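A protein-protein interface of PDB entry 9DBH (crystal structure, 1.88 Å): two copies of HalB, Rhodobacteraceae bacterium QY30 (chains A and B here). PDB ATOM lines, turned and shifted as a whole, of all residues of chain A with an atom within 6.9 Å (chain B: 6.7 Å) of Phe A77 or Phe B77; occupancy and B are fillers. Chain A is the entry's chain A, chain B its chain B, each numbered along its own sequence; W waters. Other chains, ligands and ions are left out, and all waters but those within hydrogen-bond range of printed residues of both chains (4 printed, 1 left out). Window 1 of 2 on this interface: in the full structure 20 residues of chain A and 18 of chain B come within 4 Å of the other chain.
The backbone carbonyl oxygen of Ala B76 lies close to the side-chain amino group of Lys B93, 3.5 Å away.
Among the printed residues, merely in contact across the chains: Phe A77 with Phe B77 (3.5 Å), Phe A77 with Leu B96 (3.6 Å), Lys A93 with Ile B151 (3.4 Å), Leu A96 with Ile B151 (3.9 Å), Lys A150 with Leu B96 (3.8 Å) and Ile A152 with Glu B94 (3.8 Å).
The backbone carbonyl oxygen (O) of Phe A77 is in hydrogen-bond range of the side-chain amino group (NZ) of Lys B93. O of Phe B77 is in hydrogen-bond range of NZ of Lys A93 (2.7 Å). O of Phe B77 sits close to O of Ala A76, at 3.4 Å. The backbone carbonyl oxygen (O) of Phe A77 lies close to the backbone carbonyl oxygen (O) of Ala B76, at 3.4 Å.
Hydrophobic or aromatic side chains of chain A that line the printed part of chain B: Ala A76, Phe A77, Leu A96 and Ile A152. Among the printed residues, no Asp or Glu carboxylate lies within 4 Å of a Lys or Arg side-chain nitrogen of the other chain.
Water W2 lies within hydrogen-bond range of the backbone carbonyl oxygen (O) of Leu A96 (2.7 Å), the backbone NH (N) of Ile B151 (2.8 Å) and the backbone carbonyl oxygen (O) of Lys A93 (2.8 Å). Water W1 lies within hydrogen-bond range of O of Leu B96 (2.7 Å), N of Ile A151 (2.8 Å) and O of Lys B93 (3.1 Å). Water W3 lies within hydrogen-bond range of O of Gly B79 (2.8 Å), NZ of Lys A93 (3.2 Å) and O of Glu B78 (3.5 Å). Water W4 lies within hydrogen-bond range of the backbone carbonyl oxygen of Gly A79 (2.8 Å), the side-chain amino group of Lys B93 (3.1 Å) and the backbone carbonyl oxygen of Phe A77 (3.5 Å).
Phe B77 touches its own counterpart, Phe A77. Phe A77 touches Leu B96, but with the chains exchanged Leu A96 does not touch Phe B77 (4.4 Å). Lys A93 touches Ile B151, but with the chains exchanged Ile A151 does not touch Lys B93 (4.3 Å). Leu A96 touches Ile B151, but with the chains exchanged Ile A151 does not touch Leu B96 (4.3 Å). Positions printed for both chains: 72, 73, 74, 75, 76, 77, 78, 79, 92, 93, 96, 98, 151 and 153.
Of chain B, only Ala B76 (3.4 Å), Phe B77 (3.5 Å), Lys B93 (2.9 Å) and Leu B96 (3.6 Å) come within 4 Å of Phe A77. Printed residues of chain B within 4 Å of Leu A96: Ile B151. Ala B72 touches none of the printed residues of chain A. Of the printed residues of chain A, Phe B77 touches Ala A76 (3.4 Å), Phe A77 (3.5 Å) and Lys A93 (2.7 Å). Of the printed residues of chain A, Leu B96 touches Phe A77 (3.6 Å) and Lys A150 (3.8 Å). The nearest residue of chain B that does not touch Phe A77 is Glu B94 (5.2 Å). The nearest printed residue of chain B that does not touch Ala A76 is Ala B76 (4.5 Å).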
ATOM      1  N   ALA A  72       4.450 -14.312  26.273  1.00  0.00           N
ATOM      2  CA  ALA A  72       4.889 -14.411  27.662  1.00  0.00           C
ATOM      3  C   ALA A  72       6.373 -14.100  27.799  1.00  0.00           C
ATOM      4  O   ALA A  72       6.801 -13.480  28.785  1.00  0.00           O
ATOM      5  CB  ALA A  72       4.578 -15.803  28.208  1.00  0.00           C
ATOM      6  N   ILE A  73       7.180 -14.536  26.829  1.00  0.00           N
ATOM      7  CA  ILE A  73       8.601 -14.211  26.849  1.00  0.00           C
ATOM      8  C   ILE A  73       8.791 -12.700  26.783  1.00  0.00           C
ATOM      9  O   ILE A  73       9.645 -12.134  27.476  1.00  0.00           O
ATOM     10  CB  ILE A  73       9.324 -14.933  25.692  1.00  0.00           C
ATOM     11  CG1 ILE A  73       9.178 -16.453  25.852  1.00  0.00           C
ATOM     12  CG2 ILE A  73      10.797 -14.553  25.654  1.00  0.00           C
ATOM     13  CD1 ILE A  73       9.785 -17.258  24.698  1.00  0.00           C
ATOM     14  N   HIS A  74       7.995 -12.019  25.950  1.00  0.00           N
ATOM     15  CA  HIS A  74       8.094 -10.562  25.869  1.00  0.00           C
ATOM     16  C   HIS A  74       7.817  -9.917  27.223  1.00  0.00           C
ATOM     17  O   HIS A  74       8.564  -9.040  27.671  1.00  0.00           O
ATOM     18  CB  HIS A  74       7.128 -10.004  24.829  1.00  0.00           C
ATOM     19  CG  HIS A  74       6.996  -8.512  24.902  1.00  0.00           C
ATOM     20  ND1 HIS A  74       8.032  -7.659  24.582  1.00  0.00           N
ATOM     21  CD2 HIS A  74       5.972  -7.723  25.309  1.00  0.00           C
ATOM     22  CE1 HIS A  74       7.641  -6.408  24.764  1.00  0.00           C
ATOM     23  NE2 HIS A  74       6.397  -6.421  25.207  1.00  0.00           N
ATOM     24  N   LEU A  75       6.744 -10.348  27.885  1.00  0.00           N
ATOM     25  CA  LEU A  75       6.385  -9.786  29.184  1.00  0.00           C
ATOM     26  C   LEU A  75       7.501  -9.984  30.197  1.00  0.00           C
ATOM     27  O   LEU A  75       7.829  -9.066  30.958  1.00  0.00           O
ATOM     28  CB  LEU A  75       5.095 -10.430  29.682  1.00  0.00           C
ATOM     29  CG  LEU A  75       3.882 -10.156  28.793  1.00  0.00           C
ATOM     30  CD1 LEU A  75       2.673 -10.939  29.273  1.00  0.00           C
ATOM     31  CD2 LEU A  75       3.583  -8.660  28.760  1.00  0.00           C
ATOM     32  N   ALA A  76       8.098 -11.181  30.215  1.00  0.00           N
ATOM     33  CA  ALA A  76       9.119 -11.486  31.211  1.00  0.00           C
ATOM     34  C   ALA A  76      10.411 -10.741  30.923  1.00  0.00           C
ATOM     35  O   ALA A  76      11.125 -10.346  31.851  1.00  0.00           O
ATOM     36  CB  ALA A  76       9.377 -12.995  31.255  1.00  0.00           C
ATOM     37  N   PHE A  77      10.711 -10.518  29.642  1.00  0.00           N
ATOM     38  CA  PHE A  77      11.996  -9.959  29.235  1.00  0.00           C
ATOM     39  C   PHE A  77      12.000  -8.430  29.208  1.00  0.00           C
ATOM     40  O   PHE A  77      13.043  -7.810  29.453  1.00  0.00           O
ATOM     41  CB  PHE A  77      12.351 -10.500  27.854  1.00  0.00           C
ATOM     42  CG  PHE A  77      13.749 -10.221  27.430  1.00  0.00           C
ATOM     43  CD1 PHE A  77      14.816 -10.798  28.097  1.00  0.00           C
ATOM     44  CD2 PHE A  77      14.006  -9.424  26.326  1.00  0.00           C
ATOM     45  CE1 PHE A  77      16.121 -10.563  27.684  1.00  0.00           C
ATOM     46  CE2 PHE A  77      15.311  -9.190  25.902  1.00  0.00           C
ATOM     47  CZ  PHE A  77      16.368  -9.760  26.583  1.00  0.00           C
ATOM     48  N   GLU A  78      10.871  -7.805  28.855  1.00  0.00           N
ATOM     49  CA  GLU A  78      10.797  -6.359  28.671  1.00  0.00           C
ATOM     50  C   GLU A  78       9.713  -5.672  29.491  1.00  0.00           C
ATOM     51  O   GLU A  78       9.699  -4.437  29.545  1.00  0.00           O
ATOM     52  CB  GLU A  78      10.549  -6.010  27.196  1.00  0.00           C
ATOM     53  CG  GLU A  78      11.482  -6.662  26.198  1.00  0.00           C
ATOM     54  CD  GLU A  78      11.319  -6.047  24.826  1.00  0.00           C
ATOM     55  OE1 GLU A  78      12.011  -5.053  24.523  1.00  0.00           O
ATOM     56  OE2 GLU A  78      10.462  -6.532  24.062  1.00  0.00           O
ATOM     57  N   GLY A  79       8.798  -6.420  30.096  1.00  0.00           N
ATOM     58  CA  GLY A  79       7.707  -5.799  30.818  1.00  0.00           C
ATOM     59  C   GLY A  79       8.206  -5.057  32.045  1.00  0.00           C
ATOM     60  O   GLY A  79       9.147  -5.480  32.716  1.00  0.00           O
ATOM     61  N   PHE A  92       4.804 -15.985  37.735  1.00  0.00           N
ATOM     62  CA  PHE A  92       4.798 -16.094  36.277  1.00  0.00           C
ATOM     63  C   PHE A  92       6.188 -16.422  35.737  1.00  0.00           C
ATOM     64  O   PHE A  92       6.352 -17.323  34.901  1.00  0.00           O
ATOM     65  CB  PHE A  92       4.259 -14.777  35.711  1.00  0.00           C
ATOM     66  CG  PHE A  92       4.526 -14.547  34.243  1.00  0.00           C
ATOM     67  CD1 PHE A  92       3.803 -15.212  33.270  1.00  0.00           C
ATOM     68  CD2 PHE A  92       5.439 -13.580  33.850  1.00  0.00           C
ATOM     69  CE1 PHE A  92       4.023 -14.951  31.921  1.00  0.00           C
ATOM     70  CE2 PHE A  92       5.664 -13.315  32.510  1.00  0.00           C
ATOM     71  CZ  PHE A  92       4.955 -14.001  31.541  1.00  0.00           C
ATOM     72  N   LYS A  93       7.209 -15.715  36.217  1.00  0.00           N
ATOM     73  CA  LYS A  93       8.550 -15.941  35.693  1.00  0.00           C
ATOM     74  C   LYS A  93       9.123 -17.281  36.141  1.00  0.00           C
ATOM     75  O   LYS A  93       9.917 -17.881  35.410  1.00  0.00           O
ATOM     76  CB  LYS A  93       9.467 -14.790  36.099  1.00  0.00           C
ATOM     77  CG  LYS A  93       9.079 -13.476  35.436  1.00  0.00           C
ATOM     78  CD  LYS A  93      10.051 -12.356  35.767  1.00  0.00           C
ATOM     79  CE  LYS A  93       9.615 -11.045  35.118  1.00  0.00           C
ATOM     80  NZ  LYS A  93      10.564  -9.931  35.402  1.00  0.00           N
ATOM     81  N   LEU A  96       7.993 -19.889  33.588  1.00  0.00           N
ATOM     82  CA  LEU A  96       8.356 -19.733  32.188  1.00  0.00           C
ATOM     83  C   LEU A  96       9.282 -20.859  31.743  1.00  0.00           C
ATOM     84  O   LEU A  96      10.238 -21.209  32.438  1.00  0.00           O
ATOM     85  CB  LEU A  96       9.034 -18.385  31.951  1.00  0.00           C
ATOM     86  CG  LEU A  96       9.433 -18.121  30.495  1.00  0.00           C
ATOM     87  CD1 LEU A  96       8.192 -17.969  29.617  1.00  0.00           C
ATOM     88  CD2 LEU A  96      10.338 -16.904  30.386  1.00  0.00           C
ATOM     89  N   ILE A  98      11.164 -21.472  28.146  1.00  0.00           N
ATOM     90  CA  ILE A  98      11.442 -21.041  26.782  1.00  0.00           C
ATOM     91  C   ILE A  98      11.754 -22.279  25.951  1.00  0.00           C
ATOM     92  O   ILE A  98      12.693 -23.021  26.257  1.00  0.00           O
ATOM     93  CB  ILE A  98      12.606 -20.042  26.743  1.00  0.00           C
ATOM     94  CG1 ILE A  98      12.286 -18.808  27.593  1.00  0.00           C
ATOM     95  CG2 ILE A  98      12.919 -19.653  25.296  1.00  0.00           C
ATOM     96  CD1 ILE A  98      13.510 -17.998  27.950  1.00  0.00           C
ATOM     97  N   LYS A 150      18.167 -15.716  20.912  1.00  0.00           N
ATOM     98  CA  LYS A 150      18.009 -14.275  21.043  1.00  0.00           C
ATOM     99  C   LYS A 150      16.575 -13.941  21.426  1.00  0.00           C
ATOM    100  O   LYS A 150      15.629 -14.587  20.969  1.00  0.00           O
ATOM    101  CB  LYS A 150      18.386 -13.570  19.740  1.00  0.00           C
ATOM    102  CG  LYS A 150      19.654 -14.130  19.112  1.00  0.00           C
ATOM    103  CD  LYS A 150      20.172 -13.238  17.996  1.00  0.00           C
ATOM    104  CE  LYS A 150      21.395 -13.848  17.321  1.00  0.00           C
ATOM    105  NZ  LYS A 150      21.011 -14.678  16.145  1.00  0.00           N
ATOM    106  N   ILE A 151      16.422 -12.925  22.275  1.00  0.00           N
ATOM    107  CA  ILE A 151      15.107 -12.494  22.732  1.00  0.00           C
ATOM    108  C   ILE A 151      14.805 -11.119  22.144  1.00  0.00           C
ATOM    109  O   ILE A 151      15.117 -10.085  22.745  1.00  0.00           O
ATOM    110  CB  ILE A 151      15.028 -12.478  24.271  1.00  0.00           C
ATOM    111  CG1 ILE A 151      15.660 -13.747  24.857  1.00  0.00           C
ATOM    112  CG2 ILE A 151      13.586 -12.382  24.711  1.00  0.00           C
ATOM    113  CD1 ILE A 151      14.833 -14.996  24.652  1.00  0.00           C
ATOM    114  N   ILE A 152      14.190 -11.098  20.965  1.00  0.00           N
ATOM    115  CA  ILE A 152      14.028  -9.885  20.175  1.00  0.00           C
ATOM    116  C   ILE A 152      12.546  -9.670  19.908  1.00  0.00           C
ATOM    117  O   ILE A 152      11.855 -10.588  19.453  1.00  0.00           O
ATOM    118  CB  ILE A 152      14.800  -9.973  18.846  1.00  0.00           C
ATOM    119  CG1 ILE A 152      16.269 -10.330  19.086  1.00  0.00           C
ATOM    120  CG2 ILE A 152      14.667  -8.680  18.073  1.00  0.00           C
ATOM    121  CD1 ILE A 152      17.034  -9.297  19.865  1.00  0.00           C
ATOM    122  N   PHE A 153      12.061  -8.455  20.171  1.00  0.00           N
ATOM    123  CA  PHE A 153      10.671  -8.126  19.874  1.00  0.00           C
ATOM    124  C   PHE A 153      10.459  -6.804  19.152  1.00  0.00           C
ATOM    125  O   PHE A 153       9.398  -6.637  18.543  1.00  0.00           O
ATOM    126  CB  PHE A 153       9.833  -8.125  21.162  1.00  0.00           C
ATOM    127  CG  PHE A 153       9.683  -9.488  21.769  1.00  0.00           C
ATOM    128  CD1 PHE A 153       8.676 -10.337  21.348  1.00  0.00           C
ATOM    129  CD2 PHE A 153      10.574  -9.935  22.737  1.00  0.00           C
ATOM    130  CE1 PHE A 153       8.543 -11.613  21.895  1.00  0.00           C
ATOM    131  CE2 PHE A 153      10.447 -11.214  23.288  1.00  0.00           C
ATOM    132  CZ  PHE A 153       9.429 -12.051  22.863  1.00  0.00           C
ATOM    133  N   ALA B  72      24.051 -12.224  33.558  1.00  0.00           N
ATOM    134  CA  ALA B  72      23.381 -11.295  32.653  1.00  0.00           C
ATOM    135  C   ALA B  72      21.946 -11.727  32.388  1.00  0.00           C
ATOM    136  O   ALA B  72      21.056 -10.884  32.232  1.00  0.00           O
ATOM    137  CB  ALA B  72      24.151 -11.170  31.335  1.00  0.00           C
ATOM    138  N   ILE B  73      21.700 -13.040  32.334  1.00  0.00           N
ATOM    139  CA  ILE B  73      20.334 -13.519  32.147  1.00  0.00           C
ATOM    140  C   ILE B  73      19.460 -13.095  33.325  1.00  0.00           C
ATOM    141  O   ILE B  73      18.287 -12.756  33.152  1.00  0.00           O
ATOM    142  CB  ILE B  73      20.323 -15.045  31.950  1.00  0.00           C
ATOM    143  CG1 ILE B  73      21.021 -15.419  30.639  1.00  0.00           C
ATOM    144  CG2 ILE B  73      18.899 -15.589  31.948  1.00  0.00           C
ATOM    145  CD1 ILE B  73      21.263 -16.913  30.507  1.00  0.00           C
ATOM    146  N   HIS B  74      20.015 -13.117  34.541  1.00  0.00           N
ATOM    147  CA  HIS B  74      19.266 -12.642  35.703  1.00  0.00           C
ATOM    148  C   HIS B  74      18.920 -11.165  35.564  1.00  0.00           C
ATOM    149  O   HIS B  74      17.775 -10.759  35.791  1.00  0.00           O
ATOM    150  CB  HIS B  74      20.063 -12.879  36.985  1.00  0.00           C
ATOM    151  CG  HIS B  74      19.525 -12.125  38.164  1.00  0.00           C
ATOM    152  ND1 HIS B  74      18.309 -12.425  38.748  1.00  0.00           N
ATOM    153  CD2 HIS B  74      20.025 -11.072  38.857  1.00  0.00           C
ATOM    154  CE1 HIS B  74      18.091 -11.593  39.754  1.00  0.00           C
ATOM    155  NE2 HIS B  74      19.115 -10.763  39.841  1.00  0.00           N
ATOM    156  N   LEU B  75      19.905 -10.344  35.193  1.00  0.00           N
ATOM    157  CA  LEU B  75      19.659  -8.915  35.039  1.00  0.00           C
ATOM    158  C   LEU B  75      18.581  -8.646  33.999  1.00  0.00           C
ATOM    159  O   LEU B  75      17.718  -7.783  34.200  1.00  0.00           O
ATOM    160  CB  LEU B  75      20.955  -8.201  34.658  1.00  0.00           C
ATOM    161  CG  LEU B  75      22.093  -8.299  35.675  1.00  0.00           C
ATOM    162  CD1 LEU B  75      23.348  -7.633  35.140  1.00  0.00           C
ATOM    163  CD2 LEU B  75      21.658  -7.672  36.999  1.00  0.00           C
ATOM    164  N   ALA B  76      18.603  -9.394  32.892  1.00  0.00           N
ATOM    165  CA  ALA B  76      17.685  -9.138  31.787  1.00  0.00           C
ATOM    166  C   ALA B  76      16.256  -9.542  32.131  1.00  0.00           C
ATOM    167  O   ALA B  76      15.309  -8.831  31.781  1.00  0.00           O
ATOM    168  CB  ALA B  76      18.165  -9.873  30.531  1.00  0.00           C
ATOM    169  N   PHE B  77      16.074 -10.676  32.814  1.00  0.00           N
ATOM    170  CA  PHE B  77      14.735 -11.189  33.083  1.00  0.00           C
ATOM    171  C   PHE B  77      14.177 -10.801  34.452  1.00  0.00           C
ATOM    172  O   PHE B  77      12.970 -10.971  34.674  1.00  0.00           O
ATOM    173  CB  PHE B  77      14.711 -12.719  32.957  1.00  0.00           C
ATOM    174  CG  PHE B  77      14.532 -13.219  31.538  1.00  0.00           C
ATOM    175  CD1 PHE B  77      13.292 -13.164  30.923  1.00  0.00           C
ATOM    176  CD2 PHE B  77      15.598 -13.767  30.837  1.00  0.00           C
ATOM    177  CE1 PHE B  77      13.118 -13.633  29.623  1.00  0.00           C
ATOM    178  CE2 PHE B  77      15.428 -14.241  29.532  1.00  0.00           C
ATOM    179  CZ  PHE B  77      14.188 -14.175  28.930  1.00  0.00           C
ATOM    180  N   GLU B  78      15.010 -10.306  35.376  1.00  0.00           N
ATOM    181  CA  GLU B  78      14.535  -9.935  36.710  1.00  0.00           C
ATOM    182  C   GLU B  78      14.950  -8.547  37.178  1.00  0.00           C
ATOM    183  O   GLU B  78      14.407  -8.074  38.182  1.00  0.00           O
ATOM    184  CB  GLU B  78      15.017 -10.948  37.763  1.00  0.00           C
ATOM    185  CG  GLU B  78      14.650 -12.390  37.461  1.00  0.00           C
ATOM    186  CD  GLU B  78      14.779 -13.284  38.676  1.00  0.00           C
ATOM    187  OE1 GLU B  78      15.917 -13.543  39.123  1.00  0.00           O
ATOM    188  OE2 GLU B  78      13.734 -13.723  39.196  1.00  0.00           O
ATOM    189  N   GLY B  79      15.899  -7.892  36.518  1.00  0.00           N
ATOM    190  CA  GLY B  79      16.338  -6.590  36.979  1.00  0.00           C
ATOM    191  C   GLY B  79      15.248  -5.544  36.797  1.00  0.00           C
ATOM    192  O   GLY B  79      14.471  -5.579  35.840  1.00  0.00           O
ATOM    193  N   PHE B  92      21.798  -3.642  25.886  1.00  0.00           N
ATOM    194  CA  PHE B  92      22.150  -4.845  26.637  1.00  0.00           C
ATOM    195  C   PHE B  92      21.224  -6.005  26.293  1.00  0.00           C
ATOM    196  O   PHE B  92      21.682  -7.090  25.911  1.00  0.00           O
ATOM    197  CB  PHE B  92      22.106  -4.521  28.133  1.00  0.00           C
ATOM    198  CG  PHE B  92      22.139  -5.722  29.042  1.00  0.00           C
ATOM    199  CD1 PHE B  92      23.297  -6.473  29.191  1.00  0.00           C
ATOM    200  CD2 PHE B  92      21.027  -6.063  29.790  1.00  0.00           C
ATOM    201  CE1 PHE B  92      23.332  -7.571  30.051  1.00  0.00           C
ATOM    202  CE2 PHE B  92      21.051  -7.148  30.652  1.00  0.00           C
ATOM    203  CZ  PHE B  92      22.207  -7.907  30.786  1.00  0.00           C
ATOM    204  N   LYS B  93      19.912  -5.788  26.402  1.00  0.00           N
ATOM    205  CA  LYS B  93      18.968  -6.876  26.159  1.00  0.00           C
ATOM    206  C   LYS B  93      18.970  -7.306  24.698  1.00  0.00           C
ATOM    207  O   LYS B  93      18.769  -8.486  24.399  1.00  0.00           O
ATOM    208  CB  LYS B  93      17.565  -6.462  26.602  1.00  0.00           C
ATOM    209  CG  LYS B  93      17.393  -6.535  28.109  1.00  0.00           C
ATOM    210  CD  LYS B  93      16.071  -5.957  28.578  1.00  0.00           C
ATOM    211  CE  LYS B  93      15.938  -6.115  30.091  1.00  0.00           C
ATOM    212  NZ  LYS B  93      14.607  -5.662  30.601  1.00  0.00           N
ATOM    213  N   GLU B  94      19.200  -6.372  23.775  1.00  0.00           N
ATOM    214  CA  GLU B  94      19.224  -6.752  22.366  1.00  0.00           C
ATOM    215  C   GLU B  94      20.501  -7.495  21.983  1.00  0.00           C
ATOM    216  O   GLU B  94      20.542  -8.116  20.917  1.00  0.00           O
ATOM    217  CB  GLU B  94      19.017  -5.516  21.491  1.00  0.00           C
ATOM    218  CG  GLU B  94      17.593  -4.981  21.595  1.00  0.00           C
ATOM    219  CD  GLU B  94      17.264  -3.924  20.566  1.00  0.00           C
ATOM    220  OE1 GLU B  94      18.199  -3.387  19.939  1.00  0.00           O
ATOM    221  OE2 GLU B  94      16.064  -3.630  20.382  1.00  0.00           O
ATOM    222  N   LEU B  96      21.703  -9.895  24.094  1.00  0.00           N
ATOM    223  CA  LEU B  96      21.708 -11.136  24.853  1.00  0.00           C
ATOM    224  C   LEU B  96      21.546 -12.331  23.928  1.00  0.00           C
ATOM    225  O   LEU B  96      20.659 -12.354  23.070  1.00  0.00           O
ATOM    226  CB  LEU B  96      20.595 -11.125  25.897  1.00  0.00           C
ATOM    227  CG  LEU B  96      20.532 -12.378  26.771  1.00  0.00           C
ATOM    228  CD1 LEU B  96      21.774 -12.480  27.649  1.00  0.00           C
ATOM    229  CD2 LEU B  96      19.259 -12.397  27.609  1.00  0.00           C
ATOM    230  N   ILE B  98      21.305 -16.350  24.747  1.00  0.00           N
ATOM    231  CA  ILE B  98      21.323 -17.485  25.658  1.00  0.00           C
ATOM    232  C   ILE B  98      22.042 -18.638  24.969  1.00  0.00           C
ATOM    233  O   ILE B  98      21.636 -19.082  23.891  1.00  0.00           O
ATOM    234  CB  ILE B  98      19.896 -17.856  26.080  1.00  0.00           C
ATOM    235  CG1 ILE B  98      19.237 -16.648  26.744  1.00  0.00           C
ATOM    236  CG2 ILE B  98      19.894 -19.057  27.024  1.00  0.00           C
ATOM    237  CD1 ILE B  98      17.755 -16.803  27.029  1.00  0.00           C
ATOM    238  N   ILE B 151      14.187 -19.656  33.739  1.00  0.00           N
ATOM    239  CA  ILE B 151      14.865 -18.433  34.158  1.00  0.00           C
ATOM    240  C   ILE B 151      14.797 -18.324  35.678  1.00  0.00           C
ATOM    241  O   ILE B 151      14.315 -17.322  36.221  1.00  0.00           O
ATOM    242  CB  ILE B 151      14.273 -17.177  33.473  1.00  0.00           C
ATOM    243  CG1 ILE B 151      12.772 -17.012  33.754  1.00  0.00           C
ATOM    244  CG2 ILE B 151      14.475 -17.232  31.978  1.00  0.00           C
ATOM    245  CD1 ILE B 151      12.235 -15.597  33.500  1.00  0.00           C
ATOM    246  N   PHE B 153      16.352 -18.104  39.477  1.00  0.00           N
ATOM    247  CA  PHE B 153      17.505 -17.628  40.240  1.00  0.00           C
ATOM    248  C   PHE B 153      17.295 -17.546  41.748  1.00  0.00           C
ATOM    249  O   PHE B 153      18.294 -17.489  42.473  1.00  0.00           O
ATOM    250  CB  PHE B 153      17.942 -16.247  39.738  1.00  0.00           C
ATOM    251  CG  PHE B 153      18.440 -16.259  38.323  1.00  0.00           C
ATOM    252  CD1 PHE B 153      19.762 -16.572  38.048  1.00  0.00           C
ATOM    253  CD2 PHE B 153      17.579 -15.975  37.272  1.00  0.00           C
ATOM    254  CE1 PHE B 153      20.226 -16.592  36.742  1.00  0.00           C
ATOM    255  CE2 PHE B 153      18.034 -15.998  35.958  1.00  0.00           C
ATOM    256  CZ  PHE B 153      19.362 -16.307  35.694  1.00  0.00           C
HETATM  257  O   HOH W   1      18.362 -10.981  22.663  1.00  0.00           O
HETATM  258  O   HOH W   2      11.534 -20.030  34.470  1.00  0.00           O
HETATM  259  O   HOH W   3      12.610  -7.532  35.232  1.00  0.00           O
HETATM  260  O   HOH W   4      11.827  -5.814  32.032  1.00  0.00           O
